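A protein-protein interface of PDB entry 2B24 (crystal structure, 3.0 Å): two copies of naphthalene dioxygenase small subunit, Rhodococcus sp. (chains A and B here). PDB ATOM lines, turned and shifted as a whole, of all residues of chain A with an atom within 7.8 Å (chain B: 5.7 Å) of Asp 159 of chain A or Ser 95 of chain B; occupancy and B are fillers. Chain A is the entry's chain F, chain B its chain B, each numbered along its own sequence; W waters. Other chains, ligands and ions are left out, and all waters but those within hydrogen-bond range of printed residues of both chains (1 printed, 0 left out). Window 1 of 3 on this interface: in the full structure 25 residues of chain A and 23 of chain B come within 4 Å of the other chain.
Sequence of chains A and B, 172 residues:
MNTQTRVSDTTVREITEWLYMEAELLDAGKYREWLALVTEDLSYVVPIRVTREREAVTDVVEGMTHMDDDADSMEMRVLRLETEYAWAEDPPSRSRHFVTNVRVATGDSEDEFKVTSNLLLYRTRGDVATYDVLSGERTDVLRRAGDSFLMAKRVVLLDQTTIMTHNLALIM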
ATOM      1  N   ARG A  49      -5.814   6.078 -25.601  1.00  0.00           N
ATOM      2  CA  ARG A  49      -5.122   5.668 -24.405  1.00  0.00           C
ATOM      3  C   ARG A  49      -3.757   6.319 -24.465  1.00  0.00           C
ATOM      4  O   ARG A  49      -3.210   6.487 -25.548  1.00  0.00           O
ATOM      5  CB  ARG A  49      -4.923   4.169 -24.456  1.00  0.00           C
ATOM      6  CG  ARG A  49      -6.003   3.338 -23.853  1.00  0.00           C
ATOM      7  CD  ARG A  49      -5.507   2.631 -22.641  1.00  0.00           C
ATOM      8  NE  ARG A  49      -5.459   1.192 -22.773  1.00  0.00           N
ATOM      9  CZ  ARG A  49      -5.510   0.388 -21.731  1.00  0.00           C
ATOM     10  NH1 ARG A  49      -5.629   0.895 -20.523  1.00  0.00           N
ATOM     11  NH2 ARG A  49      -5.469  -0.917 -21.882  1.00  0.00           N
ATOM     12  N   ASP A  59      -6.030   5.930 -17.538  1.00  0.00           N
ATOM     13  CA  ASP A  59      -5.261   5.785 -18.768  1.00  0.00           C
ATOM     14  C   ASP A  59      -5.941   6.483 -19.920  1.00  0.00           C
ATOM     15  O   ASP A  59      -5.294   7.023 -20.794  1.00  0.00           O
ATOM     16  CB  ASP A  59      -5.203   4.306 -19.116  1.00  0.00           C
ATOM     17  CG  ASP A  59      -3.826   3.839 -19.383  1.00  0.00           C
ATOM     18  OD1 ASP A  59      -3.691   2.720 -19.898  1.00  0.00           O
ATOM     19  OD2 ASP A  59      -2.815   4.506 -19.112  1.00  0.00           O
ATOM     20  N   ASN A 118     -13.019 -10.221 -25.069  1.00  0.00           N
ATOM     21  CA  ASN A 118     -11.674  -9.863 -25.495  1.00  0.00           C
ATOM     22  C   ASN A 118     -11.589 -10.007 -26.979  1.00  0.00           C
ATOM     23  O   ASN A 118     -11.939 -11.027 -27.506  1.00  0.00           O
ATOM     24  CB  ASN A 118     -10.651 -10.797 -24.872  1.00  0.00           C
ATOM     25  CG  ASN A 118     -10.363 -10.468 -23.460  1.00  0.00           C
ATOM     26  OD1 ASN A 118     -11.013  -9.632 -22.882  1.00  0.00           O
ATOM     27  ND2 ASN A 118      -9.385 -11.134 -22.889  1.00  0.00           N
ATOM     28  N   LEU A 119     -11.114  -8.994 -27.669  1.00  0.00           N
ATOM     29  CA  LEU A 119     -10.985  -9.092 -29.117  1.00  0.00           C
ATOM     30  C   LEU A 119      -9.520  -9.097 -29.525  1.00  0.00           C
ATOM     31  O   LEU A 119      -8.735  -8.344 -28.978  1.00  0.00           O
ATOM     32  CB  LEU A 119     -11.720  -7.943 -29.784  1.00  0.00           C
ATOM     33  CG  LEU A 119     -11.581  -7.707 -31.272  1.00  0.00           C
ATOM     34  CD1 LEU A 119     -12.592  -8.553 -31.963  1.00  0.00           C
ATOM     35  CD2 LEU A 119     -11.803  -6.249 -31.583  1.00  0.00           C
ATOM     36  N   LEU A 134      -4.905  -6.082 -33.802  1.00  0.00           N
ATOM     37  CA  LEU A 134      -5.449  -5.205 -32.784  1.00  0.00           C
ATOM     38  C   LEU A 134      -5.940  -6.061 -31.633  1.00  0.00           C
ATOM     39  O   LEU A 134      -6.601  -7.053 -31.839  1.00  0.00           O
ATOM     40  CB  LEU A 134      -6.567  -4.350 -33.361  1.00  0.00           C
ATOM     41  CG  LEU A 134      -6.180  -3.242 -34.341  1.00  0.00           C
ATOM     42  CD1 LEU A 134      -7.274  -2.233 -34.418  1.00  0.00           C
ATOM     43  CD2 LEU A 134      -4.901  -2.550 -33.945  1.00  0.00           C
ATOM     44  N   SER A 135      -5.587  -5.690 -30.417  1.00  0.00           N
ATOM     45  CA  SER A 135      -6.040  -6.404 -29.244  1.00  0.00           C
ATOM     46  C   SER A 135      -6.759  -5.413 -28.371  1.00  0.00           C
ATOM     47  O   SER A 135      -6.267  -4.321 -28.159  1.00  0.00           O
ATOM     48  CB  SER A 135      -4.845  -6.970 -28.518  1.00  0.00           C
ATOM     49  OG  SER A 135      -5.210  -7.491 -27.279  1.00  0.00           O
ATOM     50  N   GLY A 136      -7.937  -5.775 -27.886  1.00  0.00           N
ATOM     51  CA  GLY A 136      -8.729  -4.867 -27.083  1.00  0.00           C
ATOM     52  C   GLY A 136      -9.734  -5.587 -26.246  1.00  0.00           C
ATOM     53  O   GLY A 136      -9.766  -6.792 -26.299  1.00  0.00           O
ATOM     54  N   GLU A 137     -10.538  -4.859 -25.477  1.00  0.00           N
ATOM     55  CA  GLU A 137     -11.618  -5.460 -24.719  1.00  0.00           C
ATOM     56  C   GLU A 137     -12.884  -4.683 -24.931  1.00  0.00           C
ATOM     57  O   GLU A 137     -12.952  -3.525 -24.534  1.00  0.00           O
ATOM     58  CB  GLU A 137     -11.299  -5.492 -23.236  1.00  0.00           C
ATOM     59  CG  GLU A 137     -12.468  -5.963 -22.387  1.00  0.00           C
ATOM     60  CD  GLU A 137     -12.229  -5.827 -20.912  1.00  0.00           C
ATOM     61  OE1 GLU A 137     -12.033  -6.859 -20.271  1.00  0.00           O
ATOM     62  OE2 GLU A 137     -12.228  -4.702 -20.399  1.00  0.00           O
ATOM     63  N   VAL A 156     -14.848  -0.331 -27.371  1.00  0.00           N
ATOM     64  CA  VAL A 156     -13.624  -1.044 -27.690  1.00  0.00           C
ATOM     65  C   VAL A 156     -12.425  -0.334 -27.083  1.00  0.00           C
ATOM     66  O   VAL A 156     -11.963   0.668 -27.612  1.00  0.00           O
ATOM     67  CB  VAL A 156     -13.406  -1.152 -29.208  1.00  0.00           C
ATOM     68  CG1 VAL A 156     -12.332  -2.171 -29.512  1.00  0.00           C
ATOM     69  CG2 VAL A 156     -14.669  -1.495 -29.911  1.00  0.00           C
ATOM     70  N   LEU A 157     -11.917  -0.860 -25.978  1.00  0.00           N
ATOM     71  CA  LEU A 157     -10.707  -0.316 -25.377  1.00  0.00           C
ATOM     72  C   LEU A 157      -9.510  -1.178 -25.735  1.00  0.00           C
ATOM     73  O   LEU A 157      -9.326  -2.239 -25.166  1.00  0.00           O
ATOM     74  CB  LEU A 157     -10.861  -0.172 -23.865  1.00  0.00           C
ATOM     75  CG  LEU A 157      -9.818   0.596 -23.057  1.00  0.00           C
ATOM     76  CD1 LEU A 157      -9.922   2.077 -23.258  1.00  0.00           C
ATOM     77  CD2 LEU A 157      -9.958   0.267 -21.596  1.00  0.00           C
ATOM     78  N   LEU A 158      -8.707  -0.692 -26.686  1.00  0.00           N
ATOM     79  CA  LEU A 158      -7.570  -1.405 -27.248  1.00  0.00           C
ATOM     80  C   LEU A 158      -6.397  -1.401 -26.285  1.00  0.00           C
ATOM     81  O   LEU A 158      -6.316  -0.559 -25.415  1.00  0.00           O
ATOM     82  CB  LEU A 158      -7.182  -0.746 -28.569  1.00  0.00           C
ATOM     83  CG  LEU A 158      -7.596  -1.293 -29.946  1.00  0.00           C
ATOM     84  CD1 LEU A 158      -8.749  -2.287 -29.859  1.00  0.00           C
ATOM     85  CD2 LEU A 158      -7.939  -0.156 -30.907  1.00  0.00           C
ATOM     86  N   ASP A 159      -5.483  -2.341 -26.436  1.00  0.00           N
ATOM     87  CA  ASP A 159      -4.307  -2.434 -25.562  1.00  0.00           C
ATOM     88  C   ASP A 159      -3.105  -1.732 -26.131  1.00  0.00           C
ATOM     89  O   ASP A 159      -2.007  -2.259 -26.131  1.00  0.00           O
ATOM     90  CB  ASP A 159      -3.927  -3.883 -25.332  1.00  0.00           C
ATOM     91  CG  ASP A 159      -4.997  -4.637 -24.661  1.00  0.00           C
ATOM     92  OD1 ASP A 159      -5.606  -4.119 -23.702  1.00  0.00           O
ATOM     93  OD2 ASP A 159      -5.323  -5.751 -25.052  1.00  0.00           O
ATOM     94  N   GLN A 160      -3.329  -0.540 -26.639  1.00  0.00           N
ATOM     95  CA  GLN A 160      -2.305   0.168 -27.315  1.00  0.00           C
ATOM     96  C   GLN A 160      -2.612   1.587 -27.083  1.00  0.00           C
ATOM     97  O   GLN A 160      -3.767   1.946 -26.930  1.00  0.00           O
ATOM     98  CB  GLN A 160      -2.348  -0.110 -28.812  1.00  0.00           C
ATOM     99  CG  GLN A 160      -3.294  -1.181 -29.252  1.00  0.00           C
ATOM    100  CD  GLN A 160      -2.939  -1.729 -30.563  1.00  0.00           C
ATOM    101  OE1 GLN A 160      -2.763  -0.985 -31.515  1.00  0.00           O
ATOM    102  NE2 GLN A 160      -2.819  -3.034 -30.638  1.00  0.00           N
ATOM    103  N   THR A 161      -1.559   2.386 -27.039  1.00  0.00           N
ATOM    104  CA  THR A 161      -1.670   3.818 -27.148  1.00  0.00           C
ATOM    105  C   THR A 161      -1.474   4.226 -28.626  1.00  0.00           C
ATOM    106  O   THR A 161      -2.406   4.762 -29.229  1.00  0.00           O
ATOM    107  CB  THR A 161      -0.725   4.483 -26.168  1.00  0.00           C
ATOM    108  OG1 THR A 161       0.590   3.959 -26.336  1.00  0.00           O
ATOM    109  CG2 THR A 161      -1.057   4.014 -24.804  1.00  0.00           C
ATOM    110  N   THR A 162      -0.308   3.938 -29.212  1.00  0.00           N
ATOM    111  CA  THR A 162      -0.070   4.151 -30.646  1.00  0.00           C
ATOM    112  C   THR A 162      -0.687   2.985 -31.374  1.00  0.00           C
ATOM    113  O   THR A 162      -0.258   1.864 -31.196  1.00  0.00           O
ATOM    114  CB  THR A 162       1.447   4.240 -30.968  1.00  0.00           C
ATOM    115  OG1 THR A 162       1.997   5.365 -30.307  1.00  0.00           O
ATOM    116  CG2 THR A 162       1.685   4.596 -32.386  1.00  0.00           C
ATOM    117  N   ILE A 163      -1.692   3.254 -32.197  1.00  0.00           N
ATOM    118  CA  ILE A 163      -2.462   2.201 -32.863  1.00  0.00           C
ATOM    119  C   ILE A 163      -1.669   1.571 -34.005  1.00  0.00           C
ATOM    120  O   ILE A 163      -1.175   2.269 -34.887  1.00  0.00           O
ATOM    121  CB  ILE A 163      -3.826   2.749 -33.366  1.00  0.00           C
ATOM    122  CG1 ILE A 163      -4.701   3.219 -32.210  1.00  0.00           C
ATOM    123  CG2 ILE A 163      -4.551   1.723 -34.186  1.00  0.00           C
ATOM    124  CD1 ILE A 163      -4.950   2.214 -31.121  1.00  0.00           C
ATOM    125  N   MET A 164      -1.553   0.248 -33.988  1.00  0.00           N
ATOM    126  CA  MET A 164      -0.827  -0.450 -35.037  1.00  0.00           C
ATOM    127  C   MET A 164      -1.699  -0.885 -36.221  1.00  0.00           C
ATOM    128  O   MET A 164      -1.784  -2.056 -36.525  1.00  0.00           O
ATOM    129  CB  MET A 164      -0.033  -1.622 -34.448  1.00  0.00           C
ATOM    130  CG  MET A 164       1.299  -1.225 -33.793  1.00  0.00           C
ATOM    131  SD  MET A 164       1.360  -1.602 -32.044  1.00  0.00           S
ATOM    132  CE  MET A 164       2.602  -2.409 -31.944  1.00  0.00           C
ATOM    133  N   LEU B  26      -6.193  -9.673 -13.816  1.00  0.00           N
ATOM    134  CA  LEU B  26      -4.794  -9.602 -14.244  1.00  0.00           C
ATOM    135  C   LEU B  26      -4.512  -8.511 -15.288  1.00  0.00           C
ATOM    136  O   LEU B  26      -3.495  -7.806 -15.196  1.00  0.00           O
ATOM    137  CB  LEU B  26      -4.360 -10.973 -14.769  1.00  0.00           C
ATOM    138  CG  LEU B  26      -3.408 -11.827 -13.924  1.00  0.00           C
ATOM    139  CD1 LEU B  26      -3.548 -11.534 -12.451  1.00  0.00           C
ATOM    140  CD2 LEU B  26      -3.630 -13.300 -14.215  1.00  0.00           C
ATOM    141  N   ASP B  27      -5.405  -8.398 -16.276  1.00  0.00           N
ATOM    142  CA  ASP B  27      -5.355  -7.332 -17.286  1.00  0.00           C
ATOM    143  C   ASP B  27      -5.762  -5.962 -16.768  1.00  0.00           C
ATOM    144  O   ASP B  27      -5.618  -4.981 -17.477  1.00  0.00           O
ATOM    145  CB  ASP B  27      -6.286  -7.633 -18.444  1.00  0.00           C
ATOM    146  CG  ASP B  27      -6.091  -8.980 -19.010  1.00  0.00           C
ATOM    147  OD1 ASP B  27      -4.939  -9.408 -19.115  1.00  0.00           O
ATOM    148  OD2 ASP B  27      -7.051  -9.667 -19.402  1.00  0.00           O
ATOM    149  N   TYR B  31      -3.444  -7.221  -9.078  1.00  0.00           N
ATOM    150  CA  TYR B  31      -2.687  -8.396  -8.675  1.00  0.00           C
ATOM    151  C   TYR B  31      -2.969  -8.797  -7.231  1.00  0.00           C
ATOM    152  O   TYR B  31      -3.042  -9.979  -6.926  1.00  0.00           O
ATOM    153  CB  TYR B  31      -1.191  -8.164  -8.905  1.00  0.00           C
ATOM    154  CG  TYR B  31      -0.792  -8.309 -10.348  1.00  0.00           C
ATOM    155  CD1 TYR B  31      -0.775  -7.228 -11.197  1.00  0.00           C
ATOM    156  CD2 TYR B  31      -0.443  -9.532 -10.865  1.00  0.00           C
ATOM    157  CE1 TYR B  31      -0.410  -7.374 -12.539  1.00  0.00           C
ATOM    158  CE2 TYR B  31      -0.085  -9.678 -12.191  1.00  0.00           C
ATOM    159  CZ  TYR B  31      -0.074  -8.607 -13.023  1.00  0.00           C
ATOM    160  OH  TYR B  31       0.274  -8.777 -14.337  1.00  0.00           O
ATOM    161  N   SER B  93       2.230  -2.016 -18.092  1.00  0.00           N
ATOM    162  CA  SER B  93       1.977  -2.637 -19.385  1.00  0.00           C
ATOM    163  C   SER B  93       0.498  -2.648 -19.715  1.00  0.00           C
ATOM    164  O   SER B  93      -0.345  -2.497 -18.846  1.00  0.00           O
ATOM    165  CB  SER B  93       2.455  -4.072 -19.378  1.00  0.00           C
ATOM    166  OG  SER B  93       3.831  -4.136 -19.155  1.00  0.00           O
ATOM    167  N   ARG B  94       0.196  -2.808 -20.992  1.00  0.00           N
ATOM    168  CA  ARG B  94      -1.134  -3.141 -21.430  1.00  0.00           C
ATOM    169  C   ARG B  94      -1.074  -4.603 -21.799  1.00  0.00           C
ATOM    170  O   ARG B  94      -0.382  -4.994 -22.730  1.00  0.00           O
ATOM    171  CB  ARG B  94      -1.526  -2.317 -22.636  1.00  0.00           C
ATOM    172  CG  ARG B  94      -2.275  -1.070 -22.301  1.00  0.00           C
ATOM    173  CD  ARG B  94      -1.404   0.155 -22.142  1.00  0.00           C
ATOM    174  NE  ARG B  94      -0.443   0.329 -23.225  1.00  0.00           N
ATOM    175  CZ  ARG B  94       0.553   1.172 -23.173  1.00  0.00           C
ATOM    176  NH1 ARG B  94       0.725   1.907 -22.101  1.00  0.00           N
ATOM    177  NH2 ARG B  94       1.369   1.299 -24.190  1.00  0.00           N
ATOM    178  N   SER B  95      -1.774  -5.430 -21.040  1.00  0.00           N
ATOM    179  CA  SER B  95      -1.784  -6.850 -21.323  1.00  0.00           C
ATOM    180  C   SER B  95      -3.194  -7.279 -21.607  1.00  0.00           C
ATOM    181  O   SER B  95      -4.126  -6.639 -21.150  1.00  0.00           O
ATOM    182  CB  SER B  95      -1.207  -7.641 -20.151  1.00  0.00           C
ATOM    183  OG  SER B  95      -1.961  -7.492 -18.964  1.00  0.00           O
ATOM    184  N   ARG B  96      -3.344  -8.330 -22.400  1.00  0.00           N
ATOM    185  CA  ARG B  96      -4.610  -9.013 -22.577  1.00  0.00           C
ATOM    186  C   ARG B  96      -4.330 -10.498 -22.480  1.00  0.00           C
ATOM    187  O   ARG B  96      -3.480 -11.012 -23.186  1.00  0.00           O
ATOM    188  CB  ARG B  96      -5.216  -8.666 -23.929  1.00  0.00           C
ATOM    189  CG  ARG B  96      -6.694  -8.984 -24.060  1.00  0.00           C
ATOM    190  CD  ARG B  96      -7.616  -7.792 -24.111  1.00  0.00           C
ATOM    191  NE  ARG B  96      -8.213  -7.534 -22.807  1.00  0.00           N
ATOM    192  CZ  ARG B  96      -7.873  -6.540 -22.004  1.00  0.00           C
ATOM    193  NH1 ARG B  96      -6.945  -5.679 -22.351  1.00  0.00           N
ATOM    194  NH2 ARG B  96      -8.464  -6.397 -20.844  1.00  0.00           N
ATOM    195  N   HIS B  97      -5.003 -11.181 -21.568  1.00  0.00           N
ATOM    196  CA  HIS B  97      -4.817 -12.610 -21.405  1.00  0.00           C
ATOM    197  C   HIS B  97      -5.931 -13.252 -22.192  1.00  0.00           C
ATOM    198  O   HIS B  97      -7.093 -13.077 -21.857  1.00  0.00           O
ATOM    199  CB  HIS B  97      -4.933 -13.014 -19.939  1.00  0.00           C
ATOM    200  CG  HIS B  97      -3.752 -12.644 -19.093  1.00  0.00           C
ATOM    201  ND1 HIS B  97      -3.385 -11.338 -18.839  1.00  0.00           N
ATOM    202  CD2 HIS B  97      -2.890 -13.412 -18.388  1.00  0.00           C
ATOM    203  CE1 HIS B  97      -2.336 -11.318 -18.038  1.00  0.00           C
ATOM    204  NE2 HIS B  97      -2.019 -12.563 -17.744  1.00  0.00           N
ATOM    205  N   PHE B  98      -5.591 -13.962 -23.263  1.00  0.00           N
ATOM    206  CA  PHE B  98      -6.616 -14.564 -24.121  1.00  0.00           C
ATOM    207  C   PHE B  98      -6.787 -16.017 -23.726  1.00  0.00           C
ATOM    208  O   PHE B  98      -6.057 -16.878 -24.208  1.00  0.00           O
ATOM    209  CB  PHE B  98      -6.272 -14.428 -25.614  1.00  0.00           C
ATOM    210  CG  PHE B  98      -6.442 -13.041 -26.159  1.00  0.00           C
ATOM    211  CD1 PHE B  98      -5.391 -12.153 -26.177  1.00  0.00           C
ATOM    212  CD2 PHE B  98      -7.651 -12.624 -26.682  1.00  0.00           C
ATOM    213  CE1 PHE B  98      -5.551 -10.875 -26.699  1.00  0.00           C
ATOM    214  CE2 PHE B  98      -7.806 -11.341 -27.208  1.00  0.00           C
ATOM    215  CZ  PHE B  98      -6.763 -10.479 -27.203  1.00  0.00           C
ATOM    216  N   LEU B 121      -0.875 -14.256 -24.400  1.00  0.00           N
ATOM    217  CA  LEU B 121      -0.694 -12.998 -23.691  1.00  0.00           C
ATOM    218  C   LEU B 121      -0.199 -11.961 -24.672  1.00  0.00           C
ATOM    219  O   LEU B 121       0.789 -12.195 -25.355  1.00  0.00           O
ATOM    220  CB  LEU B 121       0.306 -13.171 -22.544  1.00  0.00           C
ATOM    221  CG  LEU B 121       0.656 -12.008 -21.624  1.00  0.00           C
ATOM    222  CD1 LEU B 121      -0.372 -11.829 -20.578  1.00  0.00           C
ATOM    223  CD2 LEU B 121       1.958 -12.290 -20.984  1.00  0.00           C
ATOM    224  N   TYR B 122      -0.888 -10.826 -24.743  1.00  0.00           N
ATOM    225  CA  TYR B 122      -0.502  -9.724 -25.613  1.00  0.00           C
ATOM    226  C   TYR B 122       0.008  -8.598 -24.741  1.00  0.00           C
ATOM    227  O   TYR B 122      -0.716  -8.099 -23.877  1.00  0.00           O
ATOM    228  CB  TYR B 122      -1.713  -9.258 -26.391  1.00  0.00           C
ATOM    229  CG  TYR B 122      -1.499  -8.095 -27.330  1.00  0.00           C
ATOM    230  CD1 TYR B 122      -1.300  -8.314 -28.685  1.00  0.00           C
ATOM    231  CD2 TYR B 122      -1.554  -6.779 -26.878  1.00  0.00           C
ATOM    232  CE1 TYR B 122      -1.133  -7.255 -29.553  1.00  0.00           C
ATOM    233  CE2 TYR B 122      -1.383  -5.726 -27.743  1.00  0.00           C
ATOM    234  CZ  TYR B 122      -1.172  -5.973 -29.077  1.00  0.00           C
ATOM    235  OH  TYR B 122      -1.020  -4.954 -29.972  1.00  0.00           O
ATOM    236  N   ARG B 123       1.258  -8.192 -24.963  1.00  0.00           N
ATOM    237  CA  ARG B 123       1.906  -7.200 -24.111  1.00  0.00           C
ATOM    238  C   ARG B 123       2.349  -6.009 -24.913  1.00  0.00           C
ATOM    239  O   ARG B 123       2.903  -6.166 -25.975  1.00  0.00           O
ATOM    240  CB  ARG B 123       3.111  -7.814 -23.405  1.00  0.00           C
ATOM    241  CG  ARG B 123       3.384  -7.244 -22.036  1.00  0.00           C
ATOM    242  CD  ARG B 123       4.701  -6.528 -21.926  1.00  0.00           C
ATOM    243  NE  ARG B 123       5.759  -7.310 -21.281  1.00  0.00           N
ATOM    244  CZ  ARG B 123       6.353  -6.987 -20.130  1.00  0.00           C
ATOM    245  NH1 ARG B 123       5.985  -5.923 -19.446  1.00  0.00           N
ATOM    246  NH2 ARG B 123       7.307  -7.750 -19.644  1.00  0.00           N
ATOM    247  N   THR B 124       2.106  -4.821 -24.379  1.00  0.00           N
ATOM    248  CA  THR B 124       2.495  -3.574 -25.011  1.00  0.00           C
ATOM    249  C   THR B 124       3.085  -2.610 -23.967  1.00  0.00           C
ATOM    250  O   THR B 124       2.655  -2.610 -22.814  1.00  0.00           O
ATOM    251  CB  THR B 124       1.295  -3.014 -25.733  1.00  0.00           C
ATOM    252  OG1 THR B 124       1.611  -2.888 -27.107  1.00  0.00           O
ATOM    253  CG2 THR B 124       1.019  -1.633 -25.333  1.00  0.00           C
ATOM    254  N   LEU B 170       4.727  -9.948 -15.850  1.00  0.00           N
ATOM    255  CA  LEU B 170       3.300 -10.199 -15.826  1.00  0.00           C
ATOM    256  C   LEU B 170       3.002 -11.652 -15.405  1.00  0.00           C
ATOM    257  O   LEU B 170       3.640 -12.599 -15.877  1.00  0.00           O
ATOM    258  CB  LEU B 170       2.701  -9.925 -17.208  1.00  0.00           C
ATOM    259  CG  LEU B 170       2.724  -8.521 -17.807  1.00  0.00           C
ATOM    260  CD1 LEU B 170       2.048  -8.535 -19.136  1.00  0.00           C
ATOM    261  CD2 LEU B 170       2.054  -7.508 -16.904  1.00  0.00           C
HETATM  262  O   HOH W   1      -0.290   2.944 -19.054  1.00  0.00           O
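Water W1 bridges OD2 of Asp 59 of chain A and NH1 of Arg 94 of chain B.
Among the printed residues, merely in contact across the chains: Asp 159 of chain A with Thr 124 of chain B (3.2 Å), Arg 49 of chain A with Arg 94 of chain B (3.2 Å), Gly 136 of chain A with Arg 96 of chain B (3.2 Å), Ser 135 of chain A with Phe 98 of chain B (3.4 Å), Leu 119 of chain A with Phe 98 of chain B (3.4 Å), Thr 161 of chain A with Arg 94 of chain B (3.5 Å), Asp 159 of chain A with Arg 94 of chain B (3.5 Å), Ser 135 of chain A with Arg 96 of chain B (3.6 Å), Ser 135 of chain A with Tyr 122 of chain B (3.7 Å), Asn 118 of chain A with Phe 98 of chain B (3.7 Å), Asp 159 of chain A with Tyr 122 of chain B (3.9 Å) and Asp 159 of chain A with Ser 95 of chain B (3.9 Å).
ND1 of His 97 of chain B is in hydrogen-bond range of OD1 of Asp 27 of chain B (2.5 Å). O of Arg 94 of chain B is in hydrogen-bond range of N of Thr 124 of chain B. The backbone carbonyl oxygen of Tyr 122 of chain B sits at hydrogen-bond distance from the backbone NH of Arg 96 of chain B. The backbone carbonyl oxygen (O) of Leu 119 of chain A lies within hydrogen-bond range of the backbone NH (N) of Gly 136 of chain A, 2.9 Å away. O of Ser 135 of chain A is in hydrogen-bond range of N of Asp 159 of chain A. The backbone NH (N) of Met 164 of chain A is in hydrogen-bond range of the side-chain amide oxygen (OE1) of Gln 160 of chain A, 3.0 Å away.
No position is printed for both chains. Of the 17 pairs that touch across the chains among the printed residues, none has its exchanged pair printed and touching as well.
Of the printed residues of chain B, Arg 49 of chain A touches Arg 94. Of the printed residues of chain B, Glu 137 of chain A touches Arg 96. Of chain B, only Arg 94 (3.5 Å), Ser 95 (3.9 Å), Arg 96 (2.5 Å), Tyr 122 (3.9 Å) and Thr 124 (3.2 Å) come within 4 Å of Asp 159 of chain A. Printed residues of chain B within 4 Å of Gln 160 of chain A: Tyr 122. Ile 163 of chain A touches none of the printed residues of chain B. Of the printed residues of chain A, Ser 95 of chain B touches Asp 159 (3.9 Å). Of the printed residues of chain A, His 97 of chain B touches Asn 118 (3.2 Å).
Printed residues of chain B that touch a printed residue of chain A: Arg 94, Ser 95, Arg 96, His 97, Phe 98, Tyr 122 and Thr 124. Of the 17 printed residues of chain A, 9 touch a printed residue of chain B.
The guanidinium group (NE) of Arg 96 of chain B sits at hydrogen-bond distance from the side-chain amide oxygen (OD1) of Asn 118 of chain A, at 3.5 Å. OE1 of Glu 137 of chain A is in salt-bridge range of NH2 of Arg 96 of chain B, 3.6 Å away. The guanidinium group (NH1) of Arg 96 of chain B lies within salt-bridge range of the side-chain carboxylate (OD1) of Asp 159 of chain A (2.5 Å). O of His 97 of chain B is in hydrogen-bond range of ND2 of Asn 118 of chain A, at 3.2 Å. OH of Tyr 122 of chain B lies within hydrogen-bond range of NE2 of Gln 160 of chain A (2.7 Å).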
